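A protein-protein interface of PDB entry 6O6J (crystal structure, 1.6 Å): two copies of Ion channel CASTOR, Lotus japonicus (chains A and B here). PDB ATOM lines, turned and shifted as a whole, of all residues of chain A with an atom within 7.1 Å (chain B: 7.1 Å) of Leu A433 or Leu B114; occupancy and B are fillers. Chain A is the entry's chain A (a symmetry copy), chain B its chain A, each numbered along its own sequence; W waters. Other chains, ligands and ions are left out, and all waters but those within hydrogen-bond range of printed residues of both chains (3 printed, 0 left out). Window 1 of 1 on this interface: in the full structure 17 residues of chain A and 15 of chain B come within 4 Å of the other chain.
NH1 of Arg B111 sits at hydrogen-bond distance from OG1 of Thr A429.
O of Pro B76 lies within hydrogen-bond range of OG of Ser B115 (2.7 Å).
OG1 of Thr B117 is in hydrogen-bond range of O of Leu B114, at 2.7 Å.
The backbone NH of Ile A438 is in hydrogen-bond range of the side-chain hydroxyl of Ser A436, 3.0 Å away.
Among the printed residues, merely in contact across the chains: Leu A374 with Leu B139 (3.99 Å), Arg A428 with Leu B77 (3.8 Å), Leu A432 with Arg B111 (3.9 Å), Leu A432 with Leu B114 (3.6 Å), Leu A432 with Ser B115 (3.7 Å), Leu A433 with Leu B114 (3.7 Å), Ile A438 with Leu B139 (3.7 Å) and Ile A438 with Val B143 (3.6 Å).
Leu A433 touches just one residue of chain B: Leu B114.
Leu B114 touches two residues of chain A.
Of the printed residues of chain A, Arg B111 touches Thr A429 and Leu A432.
Of the printed residues of chain B, Thr A429 touches Arg B111.
Of the printed residues of chain B, Leu A432 touches Arg B111, Leu B114 and Ser B115.
The nearest residue of chain A that does not touch Leu B114 is Ser A436 (5.0 Å).
The nearest printed residue of chain B that does not touch Leu A374 is Leu B110 (4.02 Å).
Printed residues of chain A that touch a printed residue of chain B: Leu A374, Arg A428, Thr A429, Leu A432, Leu A433 and Ile A438.
Hydrophobic or aromatic side chains of chain A within 4 Å of the printed part of chain B: Leu A374, Leu A432, Leu A433 and Ile A438.
Among the printed residues, no Asp or Glu carboxylate lies within 4 Å of a Lys or Arg side-chain nitrogen of the other chain.
No position is printed for both chains.
Of the 9 pairs that touch across the chains among the printed residues, none has its exchanged pair printed and touching as well.
Water W3 bridges O of Leu B77 (2.8 Å) and NH1 of Arg A428 (2.8 Å).
Water W2 bridges the guanidinium group (NH2) of Arg B111 (2.8 Å) and the guanidinium group (NE) of Arg A428 (3.2 Å).
Water W1 bridges O of Leu B114 (2.9 Å) and O of Leu A432 (3.3 Å).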
ATOM      1  N   LEU A 374     -17.895 -28.620 -15.918  1.00  0.00           N
ATOM      2  CA  LEU A 374     -19.218 -29.032 -16.402  1.00  0.00           C
ATOM      3  C   LEU A 374     -19.138 -30.284 -17.274  1.00  0.00           C
ATOM      4  O   LEU A 374     -20.076 -31.104 -17.285  1.00  0.00           O
ATOM      5  CB  LEU A 374     -19.880 -27.893 -17.186  1.00  0.00           C
ATOM      6  CG  LEU A 374     -20.196 -26.667 -16.346  1.00  0.00           C
ATOM      7  CD1 LEU A 374     -20.638 -25.503 -17.256  1.00  0.00           C
ATOM      8  CD2 LEU A 374     -21.280 -26.957 -15.298  1.00  0.00           C
ATOM      9  N   ILE A 424     -17.427 -23.574  -9.668  1.00  0.00           N
ATOM     10  CA  ILE A 424     -17.517 -22.677 -10.831  1.00  0.00           C
ATOM     11  C   ILE A 424     -16.847 -21.353 -10.469  1.00  0.00           C
ATOM     12  O   ILE A 424     -17.214 -20.702  -9.480  1.00  0.00           O
ATOM     13  CB  ILE A 424     -18.968 -22.473 -11.290  1.00  0.00           C
ATOM     14  CG1 ILE A 424     -19.552 -23.785 -11.836  1.00  0.00           C
ATOM     15  CG2 ILE A 424     -19.072 -21.280 -12.277  1.00  0.00           C
ATOM     16  CD1 ILE A 424     -18.931 -24.301 -13.140  1.00  0.00           C
ATOM     17  N   PRO A 427     -18.879 -16.135 -11.601  1.00  0.00           N
ATOM     18  CA  PRO A 427     -20.289 -16.033 -11.179  1.00  0.00           C
ATOM     19  C   PRO A 427     -21.258 -15.879 -12.335  1.00  0.00           C
ATOM     20  O   PRO A 427     -22.404 -16.314 -12.223  1.00  0.00           O
ATOM     21  CB  PRO A 427     -20.307 -14.780 -10.280  1.00  0.00           C
ATOM     22  CG  PRO A 427     -18.906 -14.687  -9.750  1.00  0.00           C
ATOM     23  CD  PRO A 427     -18.015 -15.163 -10.904  1.00  0.00           C
ATOM     24  N   ARG A 428     -20.829 -15.256 -13.437  1.00  0.00           N
ATOM     25  CA  ARG A 428     -21.723 -15.130 -14.587  1.00  0.00           C
ATOM     26  C   ARG A 428     -22.181 -16.492 -15.091  1.00  0.00           C
ATOM     27  O   ARG A 428     -23.336 -16.658 -15.493  1.00  0.00           O
ATOM     28  CB  ARG A 428     -21.044 -14.365 -15.723  1.00  0.00           C
ATOM     29  CG  ARG A 428     -22.041 -14.072 -16.866  1.00  0.00           C
ATOM     30  CD  ARG A 428     -21.363 -13.437 -18.073  1.00  0.00           C
ATOM     31  NE  ARG A 428     -20.640 -12.228 -17.716  1.00  0.00           N
ATOM     32  CZ  ARG A 428     -21.220 -11.035 -17.599  1.00  0.00           C
ATOM     33  NH1 ARG A 428     -22.525 -10.920 -17.798  1.00  0.00           N
ATOM     34  NH2 ARG A 428     -20.495  -9.974 -17.279  1.00  0.00           N
ATOM     35  N   THR A 429     -21.280 -17.477 -15.119  1.00  0.00           N
ATOM     36  CA  THR A 429     -21.664 -18.797 -15.591  1.00  0.00           C
ATOM     37  C   THR A 429     -22.673 -19.439 -14.648  1.00  0.00           C
ATOM     38  O   THR A 429     -23.610 -20.111 -15.093  1.00  0.00           O
ATOM     39  CB  THR A 429     -20.412 -19.675 -15.742  1.00  0.00           C
ATOM     40  OG1 THR A 429     -19.558 -19.095 -16.752  1.00  0.00           O
ATOM     41  CG2 THR A 429     -20.785 -21.127 -16.140  1.00  0.00           C
ATOM     42  N   LYS A 430     -22.503 -19.241 -13.334  1.00  0.00           N
ATOM     43  CA  LYS A 430     -23.496 -19.756 -12.407  1.00  0.00           C
ATOM     44  C   LYS A 430     -24.856 -19.124 -12.669  1.00  0.00           C
ATOM     45  O   LYS A 430     -25.879 -19.825 -12.700  1.00  0.00           O
ATOM     46  CB  LYS A 430     -23.032 -19.506 -10.958  1.00  0.00           C
ATOM     47  CG  LYS A 430     -24.005 -20.007  -9.905  1.00  0.00           C
ATOM     48  CD  LYS A 430     -24.766 -18.827  -9.310  1.00  0.00           C
ATOM     49  CE  LYS A 430     -25.806 -19.259  -8.304  1.00  0.00           C
ATOM     50  NZ  LYS A 430     -26.560 -18.052  -7.848  1.00  0.00           N
ATOM     51  N   ASN A 431     -24.885 -17.804 -12.878  1.00  0.00           N
ATOM     52  CA  ASN A 431     -26.152 -17.137 -13.144  1.00  0.00           C
ATOM     53  C   ASN A 431     -26.766 -17.633 -14.447  1.00  0.00           C
ATOM     54  O   ASN A 431     -27.988 -17.807 -14.542  1.00  0.00           O
ATOM     55  CB  ASN A 431     -25.943 -15.631 -13.189  1.00  0.00           C
ATOM     56  CG  ASN A 431     -25.645 -15.061 -11.826  1.00  0.00           C
ATOM     57  OD1 ASN A 431     -26.084 -15.607 -10.811  1.00  0.00           O
ATOM     58  ND2 ASN A 431     -24.888 -13.971 -11.788  1.00  0.00           N
ATOM     59  N   LEU A 432     -25.930 -17.882 -15.459  1.00  0.00           N
ATOM     60  CA  LEU A 432     -26.475 -18.334 -16.741  1.00  0.00           C
ATOM     61  C   LEU A 432     -27.068 -19.732 -16.636  1.00  0.00           C
ATOM     62  O   LEU A 432     -27.961 -20.093 -17.412  1.00  0.00           O
ATOM     63  CB  LEU A 432     -25.380 -18.297 -17.818  1.00  0.00           C
ATOM     64  CG  LEU A 432     -24.977 -16.921 -18.331  1.00  0.00           C
ATOM     65  CD1 LEU A 432     -23.692 -17.024 -19.117  1.00  0.00           C
ATOM     66  CD2 LEU A 432     -26.086 -16.358 -19.221  1.00  0.00           C
ATOM     67  N   LEU A 433     -26.582 -20.537 -15.698  1.00  0.00           N
ATOM     68  CA  LEU A 433     -27.097 -21.875 -15.471  1.00  0.00           C
ATOM     69  C   LEU A 433     -28.332 -21.904 -14.591  1.00  0.00           C
ATOM     70  O   LEU A 433     -28.843 -23.003 -14.341  1.00  0.00           O
ATOM     71  CB  LEU A 433     -26.013 -22.739 -14.821  1.00  0.00           C
ATOM     72  CG  LEU A 433     -24.837 -23.153 -15.686  1.00  0.00           C
ATOM     73  CD1 LEU A 433     -23.722 -23.635 -14.799  1.00  0.00           C
ATOM     74  CD2 LEU A 433     -25.288 -24.243 -16.675  1.00  0.00           C
ATOM     75  N   SER A 434     -28.839 -20.747 -14.147  1.00  0.00           N
ATOM     76  CA  SER A 434     -29.790 -20.735 -13.031  1.00  0.00           C
ATOM     77  C   SER A 434     -31.165 -21.299 -13.388  1.00  0.00           C
ATOM     78  O   SER A 434     -31.896 -21.710 -12.482  1.00  0.00           O
ATOM     79  CB  SER A 434     -29.946 -19.318 -12.480  1.00  0.00           C
ATOM     80  OG  SER A 434     -30.640 -18.490 -13.398  1.00  0.00           O
ATOM     81  N   MET A 435     -31.552 -21.316 -14.662  1.00  0.00           N
ATOM     82  CA  MET A 435     -32.817 -21.927 -15.060  1.00  0.00           C
ATOM     83  C   MET A 435     -32.657 -23.372 -15.507  1.00  0.00           C
ATOM     84  O   MET A 435     -33.638 -23.993 -15.929  1.00  0.00           O
ATOM     85  CB  MET A 435     -33.473 -21.121 -16.186  1.00  0.00           C
ATOM     86  CG  MET A 435     -33.715 -19.660 -15.840  1.00  0.00           C
ATOM     87  SD  MET A 435     -33.953 -18.654 -17.320  1.00  0.00           S
ATOM     88  CE  MET A 435     -34.116 -17.021 -16.591  1.00  0.00           C
ATOM     89  N   SER A 436     -31.451 -23.911 -15.443  1.00  0.00           N
ATOM     90  CA  SER A 436     -31.192 -25.305 -15.749  1.00  0.00           C
ATOM     91  C   SER A 436     -31.159 -26.139 -14.470  1.00  0.00           C
ATOM     92  O   SER A 436     -30.876 -25.638 -13.375  1.00  0.00           O
ATOM     93  CB  SER A 436     -29.863 -25.442 -16.497  1.00  0.00           C
ATOM     94  OG  SER A 436     -29.469 -26.802 -16.526  1.00  0.00           O
ATOM     95  N   LYS A 437     -31.449 -27.437 -14.624  1.00  0.00           N
ATOM     96  CA  LYS A 437     -31.240 -28.380 -13.523  1.00  0.00           C
ATOM     97  C   LYS A 437     -29.792 -28.361 -13.036  1.00  0.00           C
ATOM     98  O   LYS A 437     -29.529 -28.558 -11.835  1.00  0.00           O
ATOM     99  CB  LYS A 437     -31.620 -29.794 -13.967  1.00  0.00           C
ATOM    100  CG  LYS A 437     -30.919 -30.246 -15.253  1.00  0.00           C
ATOM    101  CD  LYS A 437     -30.465 -31.702 -15.182  1.00  0.00           C
ATOM    102  CE  LYS A 437     -29.704 -32.093 -16.443  1.00  0.00           C
ATOM    103  NZ  LYS A 437     -29.036 -33.420 -16.328  1.00  0.00           N
ATOM    104  N   ILE A 438     -28.851 -28.119 -13.955  1.00  0.00           N
ATOM    105  CA  ILE A 438     -27.422 -28.077 -13.643  1.00  0.00           C
ATOM    106  C   ILE A 438     -27.132 -27.176 -12.455  1.00  0.00           C
ATOM    107  O   ILE A 438     -26.157 -27.395 -11.726  1.00  0.00           O
ATOM    108  CB  ILE A 438     -26.628 -27.606 -14.885  1.00  0.00           C
ATOM    109  CG1 ILE A 438     -26.781 -28.604 -16.025  1.00  0.00           C
ATOM    110  CG2 ILE A 438     -25.154 -27.400 -14.543  1.00  0.00           C
ATOM    111  CD1 ILE A 438     -26.256 -28.073 -17.323  1.00  0.00           C
ATOM    112  N   SER A 439     -27.946 -26.137 -12.257  1.00  0.00           N
ATOM    113  CA  SER A 439     -27.666 -25.162 -11.206  1.00  0.00           C
ATOM    114  C   SER A 439     -27.623 -25.813  -9.829  1.00  0.00           C
ATOM    115  O   SER A 439     -26.977 -25.280  -8.917  1.00  0.00           O
ATOM    116  CB  SER A 439     -28.709 -24.033 -11.223  1.00  0.00           C
ATOM    117  OG  SER A 439     -30.011 -24.534 -10.968  1.00  0.00           O
ATOM    118  N   ASP A 440     -28.293 -26.958  -9.656  1.00  0.00           N
ATOM    119  CA  ASP A 440     -28.290 -27.612  -8.353  1.00  0.00           C
ATOM    120  C   ASP A 440     -26.961 -28.278  -8.044  1.00  0.00           C
ATOM    121  O   ASP A 440     -26.730 -28.675  -6.897  1.00  0.00           O
ATOM    122  CB  ASP A 440     -29.408 -28.651  -8.273  1.00  0.00           C
ATOM    123  CG  ASP A 440     -30.797 -28.022  -8.218  1.00  0.00           C
ATOM    124  OD1 ASP A 440     -30.928 -26.877  -7.730  1.00  0.00           O
ATOM    125  OD2 ASP A 440     -31.754 -28.685  -8.657  1.00  0.00           O
ATOM    126  N   VAL A 442     -23.789 -26.927  -8.723  1.00  0.00           N
ATOM    127  CA  VAL A 442     -22.673 -25.986  -8.827  1.00  0.00           C
ATOM    128  C   VAL A 442     -22.594 -25.117  -7.575  1.00  0.00           C
ATOM    129  O   VAL A 442     -23.616 -24.712  -7.009  1.00  0.00           O
ATOM    130  CB  VAL A 442     -22.789 -25.100 -10.090  1.00  0.00           C
ATOM    131  CG1 VAL A 442     -22.655 -25.941 -11.372  1.00  0.00           C
ATOM    132  CG2 VAL A 442     -24.082 -24.335 -10.106  1.00  0.00           C
ATOM    133  N   PRO B  76     -23.023 -11.451 -26.634  1.00  0.00           N
ATOM    134  CA  PRO B  76     -24.259 -12.233 -26.596  1.00  0.00           C
ATOM    135  C   PRO B  76     -24.690 -12.600 -25.171  1.00  0.00           C
ATOM    136  O   PRO B  76     -25.807 -13.088 -24.989  1.00  0.00           O
ATOM    137  CB  PRO B  76     -23.903 -13.478 -27.423  1.00  0.00           C
ATOM    138  CG  PRO B  76     -22.454 -13.632 -27.290  1.00  0.00           C
ATOM    139  CD  PRO B  76     -21.862 -12.236 -27.090  1.00  0.00           C
ATOM    140  N   LEU B  77     -23.860 -12.350 -24.160  1.00  0.00           N
ATOM    141  CA  LEU B  77     -24.233 -12.648 -22.778  1.00  0.00           C
ATOM    142  C   LEU B  77     -24.903 -11.475 -22.094  1.00  0.00           C
ATOM    143  O   LEU B  77     -25.362 -11.608 -20.945  1.00  0.00           O
ATOM    144  CB  LEU B  77     -23.003 -13.044 -21.962  1.00  0.00           C
ATOM    145  CG  LEU B  77     -22.120 -14.062 -22.652  1.00  0.00           C
ATOM    146  CD1 LEU B  77     -20.945 -14.404 -21.746  1.00  0.00           C
ATOM    147  CD2 LEU B  77     -22.965 -15.316 -23.009  1.00  0.00           C
ATOM    148  N   ARG B 108     -17.668 -20.727 -25.080  1.00  0.00           N
ATOM    149  CA  ARG B 108     -18.437 -19.542 -25.445  1.00  0.00           C
ATOM    150  C   ARG B 108     -19.807 -19.923 -25.988  1.00  0.00           C
ATOM    151  O   ARG B 108     -20.813 -19.284 -25.660  1.00  0.00           O
ATOM    152  CB  ARG B 108     -17.679 -18.690 -26.472  1.00  0.00           C
ATOM    153  CG  ARG B 108     -18.622 -17.668 -27.152  1.00  0.00           C
ATOM    154  CD  ARG B 108     -17.963 -17.024 -28.366  1.00  0.00           C
ATOM    155  NE  ARG B 108     -18.790 -16.004 -29.010  1.00  0.00           N
ATOM    156  CZ  ARG B 108     -19.533 -16.211 -30.100  1.00  0.00           C
ATOM    157  NH1 ARG B 108     -19.584 -17.412 -30.669  1.00  0.00           N
ATOM    158  NH2 ARG B 108     -20.229 -15.211 -30.627  1.00  0.00           N
ATOM    159  N   ALA B 109     -19.863 -20.961 -26.822  1.00  0.00           N
ATOM    160  CA  ALA B 109     -21.136 -21.388 -27.394  1.00  0.00           C
ATOM    161  C   ALA B 109     -22.136 -21.778 -26.309  1.00  0.00           C
ATOM    162  O   ALA B 109     -23.311 -21.411 -26.378  1.00  0.00           O
ATOM    163  CB  ALA B 109     -20.914 -22.553 -28.358  1.00  0.00           C
ATOM    164  N   LEU B 110     -21.686 -22.553 -25.309  1.00  0.00           N
ATOM    165  CA  LEU B 110     -22.565 -22.952 -24.221  1.00  0.00           C
ATOM    166  C   LEU B 110     -23.092 -21.740 -23.464  1.00  0.00           C
ATOM    167  O   LEU B 110     -24.294 -21.637 -23.213  1.00  0.00           O
ATOM    168  CB  LEU B 110     -21.817 -23.899 -23.275  1.00  0.00           C
ATOM    169  CG  LEU B 110     -22.599 -24.346 -22.039  1.00  0.00           C
ATOM    170  CD1 LEU B 110     -23.849 -25.185 -22.381  1.00  0.00           C
ATOM    171  CD2 LEU B 110     -21.644 -25.134 -21.127  1.00  0.00           C
ATOM    172  N   ARG B 111     -22.200 -20.803 -23.111  1.00  0.00           N
ATOM    173  CA  ARG B 111     -22.644 -19.606 -22.399  1.00  0.00           C
ATOM    174  C   ARG B 111     -23.625 -18.797 -23.235  1.00  0.00           C
ATOM    175  O   ARG B 111     -24.619 -18.263 -22.712  1.00  0.00           O
ATOM    176  CB  ARG B 111     -21.437 -18.760 -22.007  1.00  0.00           C
ATOM    177  CG  ARG B 111     -20.777 -19.288 -20.733  1.00  0.00           C
ATOM    178  CD  ARG B 111     -19.334 -18.915 -20.617  1.00  0.00           C
ATOM    179  NE  ARG B 111     -18.933 -17.497 -20.680  1.00  0.00           N
ATOM    180  CZ  ARG B 111     -18.843 -16.633 -19.662  1.00  0.00           C
ATOM    181  NH1 ARG B 111     -19.255 -16.929 -18.426  1.00  0.00           N
ATOM    182  NH2 ARG B 111     -18.361 -15.414 -19.902  1.00  0.00           N
ATOM    183  N   THR B 112     -23.387 -18.735 -24.549  1.00  0.00           N
ATOM    184  CA  THR B 112     -24.288 -17.981 -25.417  1.00  0.00           C
ATOM    185  C   THR B 112     -25.658 -18.630 -25.502  1.00  0.00           C
ATOM    186  O   THR B 112     -26.674 -17.931 -25.475  1.00  0.00           O
ATOM    187  CB  THR B 112     -23.672 -17.838 -26.821  1.00  0.00           C
ATOM    188  OG1 THR B 112     -22.437 -17.111 -26.749  1.00  0.00           O
ATOM    189  CG2 THR B 112     -24.653 -17.075 -27.738  1.00  0.00           C
ATOM    190  N   VAL B 113     -25.713 -19.967 -25.610  1.00  0.00           N
ATOM    191  CA  VAL B 113     -27.006 -20.642 -25.662  1.00  0.00           C
ATOM    192  C   VAL B 113     -27.760 -20.412 -24.360  1.00  0.00           C
ATOM    193  O   VAL B 113     -28.955 -20.093 -24.370  1.00  0.00           O
ATOM    194  CB  VAL B 113     -26.809 -22.142 -25.959  1.00  0.00           C
ATOM    195  CG1 VAL B 113     -28.081 -22.909 -25.720  1.00  0.00           C
ATOM    196  CG2 VAL B 113     -26.393 -22.321 -27.415  1.00  0.00           C
ATOM    197  N   LEU B 114     -27.059 -20.510 -23.220  1.00  0.00           N
ATOM    198  CA  LEU B 114     -27.728 -20.231 -21.943  1.00  0.00           C
ATOM    199  C   LEU B 114     -28.275 -18.809 -21.899  1.00  0.00           C
ATOM    200  O   LEU B 114     -29.403 -18.573 -21.427  1.00  0.00           O
ATOM    201  CB  LEU B 114     -26.752 -20.465 -20.796  1.00  0.00           C
ATOM    202  CG  LEU B 114     -26.406 -21.937 -20.588  1.00  0.00           C
ATOM    203  CD1 LEU B 114     -25.196 -22.024 -19.631  1.00  0.00           C
ATOM    204  CD2 LEU B 114     -27.620 -22.718 -20.046  1.00  0.00           C
ATOM    205  N   SER B 115     -27.496 -17.848 -22.379  1.00  0.00           N
ATOM    206  CA  SER B 115     -27.961 -16.463 -22.422  1.00  0.00           C
ATOM    207  C   SER B 115     -29.235 -16.330 -23.249  1.00  0.00           C
ATOM    208  O   SER B 115     -30.228 -15.735 -22.800  1.00  0.00           O
ATOM    209  CB  SER B 115     -26.857 -15.565 -22.981  1.00  0.00           C
ATOM    210  OG  SER B 115     -27.355 -14.245 -23.049  1.00  0.00           O
ATOM    211  N   LEU B 116     -29.228 -16.897 -24.460  1.00  0.00           N
ATOM    212  CA  LEU B 116     -30.393 -16.825 -25.348  1.00  0.00           C
ATOM    213  C   LEU B 116     -31.622 -17.493 -24.735  1.00  0.00           C
ATOM    214  O   LEU B 116     -32.755 -17.007 -24.902  1.00  0.00           O
ATOM    215  CB  LEU B 116     -30.044 -17.472 -26.702  1.00  0.00           C
ATOM    216  CG  LEU B 116     -29.015 -16.659 -27.505  1.00  0.00           C
ATOM    217  CD1 LEU B 116     -28.496 -17.511 -28.696  1.00  0.00           C
ATOM    218  CD2 LEU B 116     -29.542 -15.269 -27.974  1.00  0.00           C
ATOM    219  N   THR B 117     -31.431 -18.625 -24.048  1.00  0.00           N
ATOM    220  CA  THR B 117     -32.560 -19.278 -23.392  1.00  0.00           C
ATOM    221  C   THR B 117     -33.087 -18.441 -22.237  1.00  0.00           C
ATOM    222  O   THR B 117     -34.245 -18.619 -21.836  1.00  0.00           O
ATOM    223  CB  THR B 117     -32.185 -20.681 -22.886  1.00  0.00           C
ATOM    224  OG1 THR B 117     -31.206 -20.577 -21.844  1.00  0.00           O
ATOM    225  CG2 THR B 117     -31.684 -21.564 -23.998  1.00  0.00           C
ATOM    226  N   GLY B 118     -32.265 -17.547 -21.684  1.00  0.00           N
ATOM    227  CA  GLY B 118     -32.749 -16.655 -20.643  1.00  0.00           C
ATOM    228  C   GLY B 118     -33.532 -15.430 -21.098  1.00  0.00           C
ATOM    229  O   GLY B 118     -34.012 -14.684 -20.239  1.00  0.00           O
ATOM    230  N   VAL B 119     -33.674 -15.190 -22.403  1.00  0.00           N
ATOM    231  CA  VAL B 119     -34.373 -13.997 -22.885  1.00  0.00           C
ATOM    232  C   VAL B 119     -35.862 -14.125 -22.563  1.00  0.00           C
ATOM    233  O   VAL B 119     -36.557 -15.001 -23.082  1.00  0.00           O
ATOM    234  CB  VAL B 119     -34.138 -13.802 -24.387  1.00  0.00           C
ATOM    235  CG1 VAL B 119     -35.020 -12.684 -24.950  1.00  0.00           C
ATOM    236  CG2 VAL B 119     -32.679 -13.473 -24.650  1.00  0.00           C
ATOM    237  N   ILE B 127     -32.147 -21.456 -32.825  1.00  0.00           N
ATOM    238  CA  ILE B 127     -30.743 -21.124 -32.635  1.00  0.00           C
ATOM    239  C   ILE B 127     -29.924 -22.197 -33.353  1.00  0.00           C
ATOM    240  O   ILE B 127     -30.063 -23.384 -33.059  1.00  0.00           O
ATOM    241  CB  ILE B 127     -30.369 -21.092 -31.143  1.00  0.00           C
ATOM    242  CG1 ILE B 127     -31.269 -20.148 -30.340  1.00  0.00           C
ATOM    243  CG2 ILE B 127     -28.899 -20.688 -30.960  1.00  0.00           C
ATOM    244  CD1 ILE B 127     -31.164 -20.424 -28.819  1.00  0.00           C
ATOM    245  N   LEU B 139     -23.963 -31.451 -24.068  1.00  0.00           N
ATOM    246  CA  LEU B 139     -24.332 -30.469 -23.047  1.00  0.00           C
ATOM    247  C   LEU B 139     -25.053 -29.284 -23.667  1.00  0.00           C
ATOM    248  O   LEU B 139     -26.061 -28.801 -23.123  1.00  0.00           O
ATOM    249  CB  LEU B 139     -23.085 -30.008 -22.283  1.00  0.00           C
ATOM    250  CG  LEU B 139     -23.378 -29.018 -21.156  1.00  0.00           C
ATOM    251  CD1 LEU B 139     -24.449 -29.610 -20.226  1.00  0.00           C
ATOM    252  CD2 LEU B 139     -22.118 -28.705 -20.387  1.00  0.00           C
ATOM    253  N   VAL B 143     -29.037 -28.159 -22.558  1.00  0.00           N
ATOM    254  CA  VAL B 143     -29.515 -26.887 -22.032  1.00  0.00           C
ATOM    255  C   VAL B 143     -30.286 -26.094 -23.070  1.00  0.00           C
ATOM    256  O   VAL B 143     -31.123 -25.270 -22.693  1.00  0.00           O
ATOM    257  CB  VAL B 143     -28.372 -26.022 -21.465  1.00  0.00           C
ATOM    258  CG1 VAL B 143     -27.583 -26.800 -20.377  1.00  0.00           C
ATOM    259  CG2 VAL B 143     -27.448 -25.496 -22.565  1.00  0.00           C
ATOM    260  N   GLY B 144     -30.062 -26.333 -24.365  1.00  0.00           N
ATOM    261  CA  GLY B 144     -30.808 -25.589 -25.369  1.00  0.00           C
ATOM    262  C   GLY B 144     -32.191 -26.139 -25.669  1.00  0.00           C
ATOM    263  O   GLY B 144     -33.036 -25.417 -26.223  1.00  0.00           O
HETATM  264  O   HOH W   1     -29.835 -17.665 -18.679  1.00  0.00           O
HETATM  265  O   HOH W   2     -17.803 -13.668 -17.804  1.00  0.00           O
HETATM  266  O   HOH W   3     -24.598 -12.642 -18.505  1.00  0.00           O
